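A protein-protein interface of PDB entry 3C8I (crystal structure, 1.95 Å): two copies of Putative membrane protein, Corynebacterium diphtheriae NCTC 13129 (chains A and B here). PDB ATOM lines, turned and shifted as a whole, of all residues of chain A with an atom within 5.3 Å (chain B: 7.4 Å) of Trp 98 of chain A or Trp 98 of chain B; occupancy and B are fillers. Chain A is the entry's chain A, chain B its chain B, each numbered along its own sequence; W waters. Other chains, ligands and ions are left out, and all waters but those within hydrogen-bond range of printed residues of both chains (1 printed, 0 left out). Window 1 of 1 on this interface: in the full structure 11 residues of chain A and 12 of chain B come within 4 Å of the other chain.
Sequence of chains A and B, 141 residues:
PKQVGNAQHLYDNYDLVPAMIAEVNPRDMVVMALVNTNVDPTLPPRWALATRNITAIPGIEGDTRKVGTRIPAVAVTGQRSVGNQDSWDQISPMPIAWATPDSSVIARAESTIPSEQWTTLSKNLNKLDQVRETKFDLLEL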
ATOM      1  N   ARG A  52      21.192 -14.750  35.210  1.00  0.00           N
ATOM      2  CA  ARG A  52      22.462 -14.153  34.832  1.00  0.00           C
ATOM      3  C   ARG A  52      22.336 -12.643  34.838  1.00  0.00           C
ATOM      4  O   ARG A  52      21.418 -12.097  34.228  1.00  0.00           O
ATOM      5  CB  ARG A  52      22.890 -14.625  33.447  1.00  0.00           C
ATOM      6  CG  ARG A  52      24.273 -14.165  33.056  1.00  0.00           C
ATOM      7  CD  ARG A  52      24.639 -14.644  31.673  1.00  0.00           C
ATOM      8  NE  ARG A  52      26.048 -14.382  31.398  1.00  0.00           N
ATOM      9  CZ  ARG A  52      26.744 -14.975  30.445  1.00  0.00           C
ATOM     10  NH1 ARG A  52      26.173 -15.888  29.658  1.00  0.00           N
ATOM     11  NH2 ARG A  52      28.024 -14.650  30.281  1.00  0.00           N
ATOM     12  N   ILE A  54      23.482  -9.276  33.456  1.00  0.00           N
ATOM     13  CA  ILE A  54      24.136  -8.775  32.265  1.00  0.00           C
ATOM     14  C   ILE A  54      23.897  -7.272  32.149  1.00  0.00           C
ATOM     15  O   ILE A  54      23.125  -6.677  32.914  1.00  0.00           O
ATOM     16  CB  ILE A  54      23.640  -9.502  31.005  1.00  0.00           C
ATOM     17  CG1 ILE A  54      22.156  -9.205  30.767  1.00  0.00           C
ATOM     18  CG2 ILE A  54      23.888 -11.020  31.110  1.00  0.00           C
ATOM     19  CD1 ILE A  54      21.620  -9.678  29.451  1.00  0.00           C
ATOM     20  N   THR A  55      24.558  -6.655  31.185  1.00  0.00           N
ATOM     21  CA  THR A  55      24.448  -5.221  31.035  1.00  0.00           C
ATOM     22  C   THR A  55      23.626  -4.830  29.836  1.00  0.00           C
ATOM     23  O   THR A  55      22.814  -3.915  29.934  1.00  0.00           O
ATOM     24  CB  THR A  55      25.847  -4.568  31.034  1.00  0.00           C
ATOM     25  OG1 THR A  55      26.551  -5.006  32.209  1.00  0.00           O
ATOM     26  CG2 THR A  55      25.742  -3.078  31.101  1.00  0.00           C
ATOM     27  N   ALA A  56      23.790  -5.528  28.720  1.00  0.00           N
ATOM     28  CA  ALA A  56      23.153  -5.113  27.483  1.00  0.00           C
ATOM     29  C   ALA A  56      22.908  -6.273  26.537  1.00  0.00           C
ATOM     30  O   ALA A  56      23.644  -7.272  26.532  1.00  0.00           O
ATOM     31  CB  ALA A  56      24.016  -4.030  26.777  1.00  0.00           C
ATOM     32  N   ILE A  57      21.863  -6.144  25.733  1.00  0.00           N
ATOM     33  CA  ILE A  57      21.591  -7.098  24.676  1.00  0.00           C
ATOM     34  C   ILE A  57      21.223  -6.303  23.429  1.00  0.00           C
ATOM     35  O   ILE A  57      20.318  -5.463  23.497  1.00  0.00           O
ATOM     36  CB  ILE A  57      20.409  -8.024  25.046  1.00  0.00           C
ATOM     37  CG1 ILE A  57      20.680  -8.779  26.358  1.00  0.00           C
ATOM     38  CG2 ILE A  57      20.119  -8.993  23.930  1.00  0.00           C
ATOM     39  CD1 ILE A  57      19.493  -9.609  26.822  1.00  0.00           C
ATOM     40  N   PRO A  58      21.886  -6.570  22.295  1.00  0.00           N
ATOM     41  CA  PRO A  58      21.526  -5.888  21.048  1.00  0.00           C
ATOM     42  C   PRO A  58      20.054  -6.073  20.706  1.00  0.00           C
ATOM     43  O   PRO A  58      19.560  -7.220  20.667  1.00  0.00           O
ATOM     44  CB  PRO A  58      22.405  -6.571  20.011  1.00  0.00           C
ATOM     45  CG  PRO A  58      23.554  -7.027  20.761  1.00  0.00           C
ATOM     46  CD  PRO A  58      23.022  -7.473  22.084  1.00  0.00           C
ATOM     47  N   MET A  94      22.868 -17.753  27.566  1.00  0.00           N
ATOM     48  CA  MET A  94      23.524 -16.748  26.751  1.00  0.00           C
ATOM     49  C   MET A  94      22.521 -16.238  25.726  1.00  0.00           C
ATOM     50  O   MET A  94      22.055 -17.011  24.879  1.00  0.00           O
ATOM     51  CB  MET A  94      24.742 -17.358  26.053  1.00  0.00           C
ATOM     52  CG  MET A  94      25.462 -16.394  25.134  1.00  0.00           C
ATOM     53  SD  MET A  94      26.796 -17.236  24.204  1.00  0.00           S
ATOM     54  CE  MET A  94      25.833 -17.624  22.780  1.00  0.00           C
ATOM     55  N   PRO A  95      22.177 -14.937  25.782  1.00  0.00           N
ATOM     56  CA  PRO A  95      21.299 -14.435  24.746  1.00  0.00           C
ATOM     57  C   PRO A  95      21.821 -14.714  23.335  1.00  0.00           C
ATOM     58  O   PRO A  95      22.985 -14.478  23.014  1.00  0.00           O
ATOM     59  CB  PRO A  95      21.248 -12.942  25.012  1.00  0.00           C
ATOM     60  CG  PRO A  95      21.566 -12.807  26.465  1.00  0.00           C
ATOM     61  CD  PRO A  95      22.536 -13.906  26.761  1.00  0.00           C
ATOM     62  N   ILE A  96      20.940 -15.229  22.494  1.00  0.00           N
ATOM     63  CA  ILE A  96      21.263 -15.441  21.087  1.00  0.00           C
ATOM     64  C   ILE A  96      21.672 -14.132  20.395  1.00  0.00           C
ATOM     65  O   ILE A  96      22.580 -14.134  19.556  1.00  0.00           O
ATOM     66  CB  ILE A  96      20.062 -16.119  20.357  1.00  0.00           C
ATOM     67  CG1 ILE A  96      19.934 -17.583  20.823  1.00  0.00           C
ATOM     68  CG2 ILE A  96      20.202 -16.039  18.841  1.00  0.00           C
ATOM     69  CD1 ILE A  96      18.619 -18.208  20.291  1.00  0.00           C
ATOM     70  N   ALA A  97      21.024 -13.023  20.754  1.00  0.00           N
ATOM     71  CA  ALA A  97      21.353 -11.702  20.191  1.00  0.00           C
ATOM     72  C   ALA A  97      22.840 -11.266  20.409  1.00  0.00           C
ATOM     73  O   ALA A  97      23.364 -10.457  19.638  1.00  0.00           O
ATOM     74  CB  ALA A  97      20.383 -10.666  20.703  1.00  0.00           C
ATOM     75  N   TRP A  98      23.511 -11.802  21.443  1.00  0.00           N
ATOM     76  CA  TRP A  98      24.949 -11.638  21.583  1.00  0.00           C
ATOM     77  C   TRP A  98      25.727 -12.153  20.382  1.00  0.00           C
ATOM     78  O   TRP A  98      26.792 -11.589  20.072  1.00  0.00           O
ATOM     79  CB  TRP A  98      25.488 -12.272  22.863  1.00  0.00           C
ATOM     80  CG  TRP A  98      25.210 -11.500  24.119  1.00  0.00           C
ATOM     81  CD1 TRP A  98      24.530 -10.328  24.248  1.00  0.00           C
ATOM     82  CD2 TRP A  98      25.609 -11.876  25.429  1.00  0.00           C
ATOM     83  NE1 TRP A  98      24.504  -9.945  25.569  1.00  0.00           N
ATOM     84  CE2 TRP A  98      25.149 -10.886  26.313  1.00  0.00           C
ATOM     85  CE3 TRP A  98      26.297 -12.970  25.944  1.00  0.00           C
ATOM     86  CZ2 TRP A  98      25.377 -10.942  27.696  1.00  0.00           C
ATOM     87  CZ3 TRP A  98      26.528 -13.020  27.316  1.00  0.00           C
ATOM     88  CH2 TRP A  98      26.058 -12.002  28.174  1.00  0.00           C
ATOM     89  N   ALA A  99      25.242 -13.208  19.722  1.00  0.00           N
ATOM     90  CA  ALA A  99      25.873 -13.705  18.513  1.00  0.00           C
ATOM     91  C   ALA A  99      25.413 -12.900  17.298  1.00  0.00           C
ATOM     92  O   ALA A  99      26.241 -12.477  16.494  1.00  0.00           O
ATOM     93  CB  ALA A  99      25.585 -15.191  18.314  1.00  0.00           C
ATOM     94  N   THR A 100      24.101 -12.713  17.167  1.00  0.00           N
ATOM     95  CA  THR A 100      23.503 -11.851  16.134  1.00  0.00           C
ATOM     96  C   THR A 100      22.115 -11.391  16.541  1.00  0.00           C
ATOM     97  O   THR A 100      21.308 -12.213  17.006  1.00  0.00           O
ATOM     98  CB  THR A 100      23.402 -12.524  14.742  1.00  0.00           C
ATOM     99  OG1 THR A 100      22.641 -11.672  13.871  1.00  0.00           O
ATOM    100  CG2 THR A 100      22.763 -13.865  14.801  1.00  0.00           C
ATOM    101  N   ARG B  52      32.088  -6.125  13.069  1.00  0.00           N
ATOM    102  CA  ARG B  52      30.703  -6.185  13.473  1.00  0.00           C
ATOM    103  C   ARG B  52      30.139  -4.795  13.681  1.00  0.00           C
ATOM    104  O   ARG B  52      30.746  -3.963  14.344  1.00  0.00           O
ATOM    105  CB  ARG B  52      30.574  -6.954  14.786  1.00  0.00           C
ATOM    106  CG  ARG B  52      29.169  -7.104  15.282  1.00  0.00           C
ATOM    107  CD  ARG B  52      29.107  -7.935  16.573  1.00  0.00           C
ATOM    108  NE  ARG B  52      27.732  -8.105  17.037  1.00  0.00           N
ATOM    109  CZ  ARG B  52      27.302  -9.076  17.837  1.00  0.00           C
ATOM    110  NH1 ARG B  52      28.156  -9.968  18.319  1.00  0.00           N
ATOM    111  NH2 ARG B  52      26.008  -9.140  18.185  1.00  0.00           N
ATOM    112  N   ASN B  53      28.953  -4.590  13.140  1.00  0.00           N
ATOM    113  CA  ASN B  53      28.211  -3.358  13.329  1.00  0.00           C
ATOM    114  C   ASN B  53      27.459  -3.416  14.645  1.00  0.00           C
ATOM    115  O   ASN B  53      26.708  -4.365  14.906  1.00  0.00           O
ATOM    116  CB  ASN B  53      27.288  -3.125  12.150  1.00  0.00           C
ATOM    117  CG  ASN B  53      28.014  -2.509  10.965  1.00  0.00           C
ATOM    118  OD1 ASN B  53      27.850  -1.315  10.678  1.00  0.00           O
ATOM    119  ND2 ASN B  53      28.826  -3.303  10.275  1.00  0.00           N
ATOM    120  N   ILE B  54      27.706  -2.435  15.499  1.00  0.00           N
ATOM    121  CA  ILE B  54      27.167  -2.410  16.860  1.00  0.00           C
ATOM    122  C   ILE B  54      26.480  -1.081  17.152  1.00  0.00           C
ATOM    123  O   ILE B  54      26.998  -0.010  16.814  1.00  0.00           O
ATOM    124  CB  ILE B  54      28.294  -2.687  17.906  1.00  0.00           C
ATOM    125  CG1 ILE B  54      28.802  -4.134  17.755  1.00  0.00           C
ATOM    126  CG2 ILE B  54      27.801  -2.453  19.354  1.00  0.00           C
ATOM    127  CD1 ILE B  54      30.034  -4.447  18.683  1.00  0.00           C
ATOM    128  N   THR B  55      25.300  -1.138  17.757  1.00  0.00           N
ATOM    129  CA  THR B  55      24.565   0.099  18.031  1.00  0.00           C
ATOM    130  C   THR B  55      24.992   0.729  19.360  1.00  0.00           C
ATOM    131  O   THR B  55      25.196   1.938  19.426  1.00  0.00           O
ATOM    132  CB  THR B  55      23.047  -0.158  17.973  1.00  0.00           C
ATOM    133  OG1 THR B  55      22.702  -0.557  16.629  1.00  0.00           O
ATOM    134  CG2 THR B  55      22.284   1.078  18.363  1.00  0.00           C
ATOM    135  N   ALA B  56      25.161  -0.082  20.402  1.00  0.00           N
ATOM    136  CA  ALA B  56      25.419   0.434  21.748  1.00  0.00           C
ATOM    137  C   ALA B  56      26.401  -0.428  22.540  1.00  0.00           C
ATOM    138  O   ALA B  56      26.278  -1.650  22.574  1.00  0.00           O
ATOM    139  CB  ALA B  56      24.116   0.553  22.524  1.00  0.00           C
ATOM    140  N   ILE B  57      27.358   0.226  23.193  1.00  0.00           N
ATOM    141  CA  ILE B  57      28.222  -0.444  24.163  1.00  0.00           C
ATOM    142  C   ILE B  57      28.263   0.448  25.407  1.00  0.00           C
ATOM    143  O   ILE B  57      28.681   1.600  25.306  1.00  0.00           O
ATOM    144  CB  ILE B  57      29.671  -0.609  23.649  1.00  0.00           C
ATOM    145  CG1 ILE B  57      29.711  -1.347  22.294  1.00  0.00           C
ATOM    146  CG2 ILE B  57      30.504  -1.324  24.702  1.00  0.00           C
ATOM    147  CD1 ILE B  57      31.088  -1.446  21.677  1.00  0.00           C
ATOM    148  N   PRO B  58      27.808  -0.068  26.567  1.00  0.00           N
ATOM    149  CA  PRO B  58      27.885   0.684  27.808  1.00  0.00           C
ATOM    150  C   PRO B  58      29.273   1.274  28.034  1.00  0.00           C
ATOM    151  O   PRO B  58      30.264   0.570  27.868  1.00  0.00           O
ATOM    152  CB  PRO B  58      27.562  -0.367  28.870  1.00  0.00           C
ATOM    153  CG  PRO B  58      26.670  -1.303  28.195  1.00  0.00           C
ATOM    154  CD  PRO B  58      27.169  -1.378  26.782  1.00  0.00           C
ATOM    155  N   PRO B  72      37.643  -4.505  24.953  1.00  0.00           N
ATOM    156  CA  PRO B  72      37.888  -5.915  25.238  1.00  0.00           C
ATOM    157  C   PRO B  72      36.663  -6.768  24.869  1.00  0.00           C
ATOM    158  O   PRO B  72      35.540  -6.392  25.185  1.00  0.00           O
ATOM    159  CB  PRO B  72      38.126  -5.931  26.747  1.00  0.00           C
ATOM    160  CG  PRO B  72      38.363  -4.545  27.114  1.00  0.00           C
ATOM    161  CD  PRO B  72      37.673  -3.682  26.161  1.00  0.00           C
ATOM    162  N   VAL B  74      35.061 -10.980  23.507  1.00  0.00           N
ATOM    163  CA  VAL B  74      35.236 -12.417  23.355  1.00  0.00           C
ATOM    164  C   VAL B  74      34.576 -12.887  22.062  1.00  0.00           C
ATOM    165  O   VAL B  74      33.621 -12.260  21.574  1.00  0.00           O
ATOM    166  CB  VAL B  74      34.714 -13.268  24.570  1.00  0.00           C
ATOM    167  CG1 VAL B  74      35.318 -12.773  25.896  1.00  0.00           C
ATOM    168  CG2 VAL B  74      33.180 -13.338  24.611  1.00  0.00           C
ATOM    169  N   VAL B  76      32.199 -15.077  20.602  1.00  0.00           N
ATOM    170  CA  VAL B  76      31.067 -15.727  21.254  1.00  0.00           C
ATOM    171  C   VAL B  76      30.591 -16.937  20.468  1.00  0.00           C
ATOM    172  O   VAL B  76      30.234 -17.957  21.080  1.00  0.00           O
ATOM    173  CB  VAL B  76      29.938 -14.730  21.620  1.00  0.00           C
ATOM    174  CG1 VAL B  76      29.183 -14.265  20.406  1.00  0.00           C
ATOM    175  CG2 VAL B  76      28.987 -15.346  22.669  1.00  0.00           C
ATOM    176  N   THR B  77      30.652 -16.875  19.139  1.00  0.00           N
ATOM    177  CA  THR B  77      30.219 -17.993  18.308  1.00  0.00           C
ATOM    178  C   THR B  77      31.037 -17.957  17.058  1.00  0.00           C
ATOM    179  O   THR B  77      31.673 -16.919  16.753  1.00  0.00           O
ATOM    180  CB  THR B  77      28.695 -17.920  17.891  1.00  0.00           C
ATOM    181  OG1 THR B  77      28.421 -16.673  17.235  1.00  0.00           O
ATOM    182  CG2 THR B  77      27.777 -18.059  19.100  1.00  0.00           C
ATOM    183  N   SER B  92      31.719 -14.306  15.410  1.00  0.00           N
ATOM    184  CA  SER B  92      31.062 -13.132  16.028  1.00  0.00           C
ATOM    185  C   SER B  92      31.762 -12.681  17.303  1.00  0.00           C
ATOM    186  O   SER B  92      31.723 -13.403  18.317  1.00  0.00           O
ATOM    187  CB  SER B  92      29.604 -13.403  16.391  1.00  0.00           C
ATOM    188  OG  SER B  92      28.874 -13.748  15.246  1.00  0.00           O
ATOM    189  N   PRO B  93      32.393 -11.502  17.259  1.00  0.00           N
ATOM    190  CA  PRO B  93      32.934 -10.933  18.490  1.00  0.00           C
ATOM    191  C   PRO B  93      31.850 -10.171  19.251  1.00  0.00           C
ATOM    192  O   PRO B  93      30.953  -9.607  18.628  1.00  0.00           O
ATOM    193  CB  PRO B  93      34.016  -9.983  17.991  1.00  0.00           C
ATOM    194  CG  PRO B  93      33.530  -9.525  16.628  1.00  0.00           C
ATOM    195  CD  PRO B  93      32.626 -10.612  16.091  1.00  0.00           C
ATOM    196  N   MET B  94      31.931 -10.170  20.572  1.00  0.00           N
ATOM    197  CA  MET B  94      31.064  -9.333  21.413  1.00  0.00           C
ATOM    198  C   MET B  94      31.900  -8.589  22.447  1.00  0.00           C
ATOM    199  O   MET B  94      32.855  -9.144  22.989  1.00  0.00           O
ATOM    200  CB  MET B  94      29.994 -10.183  22.137  1.00  0.00           C
ATOM    201  CG  MET B  94      30.514 -11.234  23.108  1.00  0.00           C
ATOM    202  SD  MET B  94      29.225 -11.944  24.245  1.00  0.00           S
ATOM    203  CE  MET B  94      28.938 -10.590  25.378  1.00  0.00           C
ATOM    204  N   PRO B  95      31.543  -7.325  22.736  1.00  0.00           N
ATOM    205  CA  PRO B  95      32.184  -6.608  23.818  1.00  0.00           C
ATOM    206  C   PRO B  95      31.863  -7.213  25.176  1.00  0.00           C
ATOM    207  O   PRO B  95      30.700  -7.532  25.443  1.00  0.00           O
ATOM    208  CB  PRO B  95      31.600  -5.199  23.740  1.00  0.00           C
ATOM    209  CG  PRO B  95      30.564  -5.228  22.716  1.00  0.00           C
ATOM    210  CD  PRO B  95      30.525  -6.538  22.034  1.00  0.00           C
ATOM    211  N   ILE B  96      32.872  -7.349  26.036  1.00  0.00           N
ATOM    212  CA  ILE B  96      32.615  -7.928  27.373  1.00  0.00           C
ATOM    213  C   ILE B  96      31.749  -6.979  28.213  1.00  0.00           C
ATOM    214  O   ILE B  96      31.022  -7.424  29.106  1.00  0.00           O
ATOM    215  CB  ILE B  96      33.889  -8.401  28.150  1.00  0.00           C
ATOM    216  CG1 ILE B  96      34.721  -7.248  28.663  1.00  0.00           C
ATOM    217  CG2 ILE B  96      34.748  -9.328  27.327  1.00  0.00           C
ATOM    218  CD1 ILE B  96      35.765  -7.711  29.722  1.00  0.00           C
ATOM    219  N   ALA B  97      31.776  -5.694  27.876  1.00  0.00           N
ATOM    220  CA  ALA B  97      30.901  -4.698  28.502  1.00  0.00           C
ATOM    221  C   ALA B  97      29.390  -5.011  28.389  1.00  0.00           C
ATOM    222  O   ALA B  97      28.609  -4.382  29.097  1.00  0.00           O
ATOM    223  CB  ALA B  97      31.185  -3.324  27.955  1.00  0.00           C
ATOM    224  N   TRP B  98      28.978  -5.924  27.507  1.00  0.00           N
ATOM    225  CA  TRP B  98      27.568  -6.336  27.429  1.00  0.00           C
ATOM    226  C   TRP B  98      27.231  -7.322  28.551  1.00  0.00           C
ATOM    227  O   TRP B  98      26.068  -7.478  28.912  1.00  0.00           O
ATOM    228  CB  TRP B  98      27.249  -7.021  26.105  1.00  0.00           C
ATOM    229  CG  TRP B  98      27.195  -6.132  24.888  1.00  0.00           C
ATOM    230  CD1 TRP B  98      27.205  -4.766  24.851  1.00  0.00           C
ATOM    231  CD2 TRP B  98      27.066  -6.573  23.536  1.00  0.00           C
ATOM    232  NE1 TRP B  98      27.121  -4.324  23.543  1.00  0.00           N
ATOM    233  CE2 TRP B  98      27.039  -5.416  22.714  1.00  0.00           C
ATOM    234  CE3 TRP B  98      27.010  -7.832  22.931  1.00  0.00           C
ATOM    235  CZ2 TRP B  98      26.942  -5.491  21.318  1.00  0.00           C
ATOM    236  CZ3 TRP B  98      26.924  -7.906  21.559  1.00  0.00           C
ATOM    237  CH2 TRP B  98      26.904  -6.742  20.761  1.00  0.00           C
ATOM    238  N   ALA B  99      28.268  -7.977  29.074  1.00  0.00           N
ATOM    239  CA  ALA B  99      28.159  -8.988  30.132  1.00  0.00           C
ATOM    240  C   ALA B  99      28.441  -8.483  31.553  1.00  0.00           C
ATOM    241  O   ALA B  99      27.969  -9.104  32.513  1.00  0.00           O
ATOM    242  CB  ALA B  99      29.090 -10.145  29.825  1.00  0.00           C
ATOM    243  N   THR B 100      29.219  -7.410  31.712  1.00  0.00           N
ATOM    244  CA  THR B 100      29.548  -6.885  33.055  1.00  0.00           C
ATOM    245  C   THR B 100      29.551  -5.355  33.147  1.00  0.00           C
ATOM    246  O   THR B 100      30.156  -4.696  32.308  1.00  0.00           O
ATOM    247  CB  THR B 100      30.944  -7.397  33.551  1.00  0.00           C
ATOM    248  OG1 THR B 100      31.301  -6.708  34.764  1.00  0.00           O
ATOM    249  CG2 THR B 100      32.042  -7.143  32.510  1.00  0.00           C
ATOM    250  N   PRO B 101      28.914  -4.780  34.201  1.00  0.00           N
ATOM    251  CA  PRO B 101      28.929  -3.324  34.391  1.00  0.00           C
ATOM    252  C   PRO B 101      30.212  -2.829  35.055  1.00  0.00           C
ATOM    253  O   PRO B 101      30.465  -1.610  35.127  1.00  0.00           O
ATOM    254  CB  PRO B 101      27.755  -3.098  35.342  1.00  0.00           C
ATOM    255  CG  PRO B 101      27.744  -4.319  36.171  1.00  0.00           C
ATOM    256  CD  PRO B 101      28.135  -5.441  35.265  1.00  0.00           C
ATOM    257  N   ILE B 106      36.520  -4.919  33.226  1.00  0.00           N
ATOM    258  CA  ILE B 106      36.723  -4.520  31.833  1.00  0.00           C
ATOM    259  C   ILE B 106      38.138  -3.967  31.662  1.00  0.00           C
ATOM    260  O   ILE B 106      38.812  -4.270  30.681  1.00  0.00           O
ATOM    261  CB  ILE B 106      35.681  -3.472  31.367  1.00  0.00           C
ATOM    262  CG1 ILE B 106      34.281  -4.098  31.316  1.00  0.00           C
ATOM    263  CG2 ILE B 106      36.050  -2.923  29.982  1.00  0.00           C
ATOM    264  CD1 ILE B 106      33.168  -3.092  31.194  1.00  0.00           C
HETATM  265  O   HOH W   1      27.331 -12.199  32.601  1.00  0.00           O
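Arg 52 of chain A touches none of the printed residues of chain B.
Of the printed residues of chain A, Val 76 of chain B touches Met 94 (3.3 Å), Trp 98 (3.6 Å) and Ala 99 (3.9 Å).
Pro 93 of chain B touches none of the printed residues of chain A.
Printed residues of chain A within 4 Å of Ala 97 of chain B: Thr 55 (3.4 Å).
Of chain A, only Ile 54, Thr 55, Ala 56, Pro 58 and Trp 98 come within 4 Å of Trp 98 of chain B.
The nearest residue of chain A that does not touch Trp 98 of chain B is Ala 97 of chain A (4.8 Å).
Among the printed residues, pairs that only touch across the chains: Thr 55 of chain A with Thr 100 of chain B, Met 94 of chain A with Val 76 of chain B, Pro 58 of chain A with Trp 98 of chain B, Ala 99 of chain A with Thr 77 of chain B, Thr 55 of chain A with Ala 97 of chain B, Thr 55 of chain A with Pro 58 of chain B, Trp 98 of chain A with Met 94 of chain B, Trp 98 of chain A with Val 76 of chain B, Ala 99 of chain A with Arg 52 of chain B, Trp 98 of chain A with Trp 98 of chain B, Ile 54 of chain A with Trp 98 of chain B, Ala 99 of chain A with Val 76 of chain B, Ile 54 of chain A with Ala 99 of chain B and Trp 98 of chain A with Ala 99 of chain B.
N of Thr 55 of chain A lies within hydrogen-bond range of O of Trp 98 of chain B, at 2.9 Å.
The backbone carbonyl oxygen (O) of Trp 98 of chain B lies within hydrogen-bond range of the backbone NH (N) of Ala 56 of chain A (3.0 Å).
The backbone carbonyl oxygen (O) of Ala 97 of chain A is in hydrogen-bond range of the guanidinium group (NH2) of Arg 52 of chain B, 3.3 Å away.
O of Trp 98 of chain A is in hydrogen-bond range of NH1 of Arg 52 of chain B (2.7 Å).
O of Ala 99 of chain A lies within hydrogen-bond range of OG of Ser 92 of chain B (3.2 Å).
OG1 of Thr 55 of chain A lies close to N of Pro 101 of chain B (3.1 Å).
Ile 54 of chain A touches Ala 99 of chain B, but with the chains exchanged Ala 99 of chain A does not touch Ile 54 of chain B (8.8 Å).
Pro 58 of chain A touches Trp 98 of chain B, but with the chains exchanged Trp 98 of chain A does not touch Pro 58 of chain B (9.1 Å).
Ala 97 of chain A touches Arg 52 of chain B, but with the chains exchanged Arg 52 of chain A does not touch Ala 97 of chain B (9.9 Å).
Trp 98 of chain A touches Arg 52 of chain B, but with the chains exchanged Arg 52 of chain A does not touch Trp 98 of chain B (7.3 Å).
Of the 22 printed residues of chain B, 11 touch a printed residue of chain A.
Among the printed residues, 20 pairs touch across the chains.
The indole nitrogen (NE1) of Trp 98 of chain A lies within hydrogen-bond range of the backbone carbonyl oxygen (O) of Ala 56 of chain A (3.0 Å).
The guanidinium group (NH1) of Arg 52 of chain B sits at hydrogen-bond distance from the backbone carbonyl oxygen (O) of Pro 93 of chain B, 2.8 Å away.
The indole nitrogen of Trp 98 of chain B is in hydrogen-bond range of the backbone carbonyl oxygen of Ala 56 of chain B (3.0 Å).
The backbone carbonyl oxygen of Val 74 of chain B sits at hydrogen-bond distance from the backbone NH of Met 94 of chain B.
O of Ser 92 of chain B is in hydrogen-bond range of N of Val 76 of chain B, 2.9 Å away.
The backbone NH (N) of Ser 92 of chain B is in hydrogen-bond range of the backbone carbonyl oxygen (O) of Thr 77 of chain B, at 2.9 Å.
Water W1 bridges the guanidinium group of Arg 52 of chain A (2.8 Å) and the backbone carbonyl oxygen of Ala 99 of chain B (3.2 Å).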
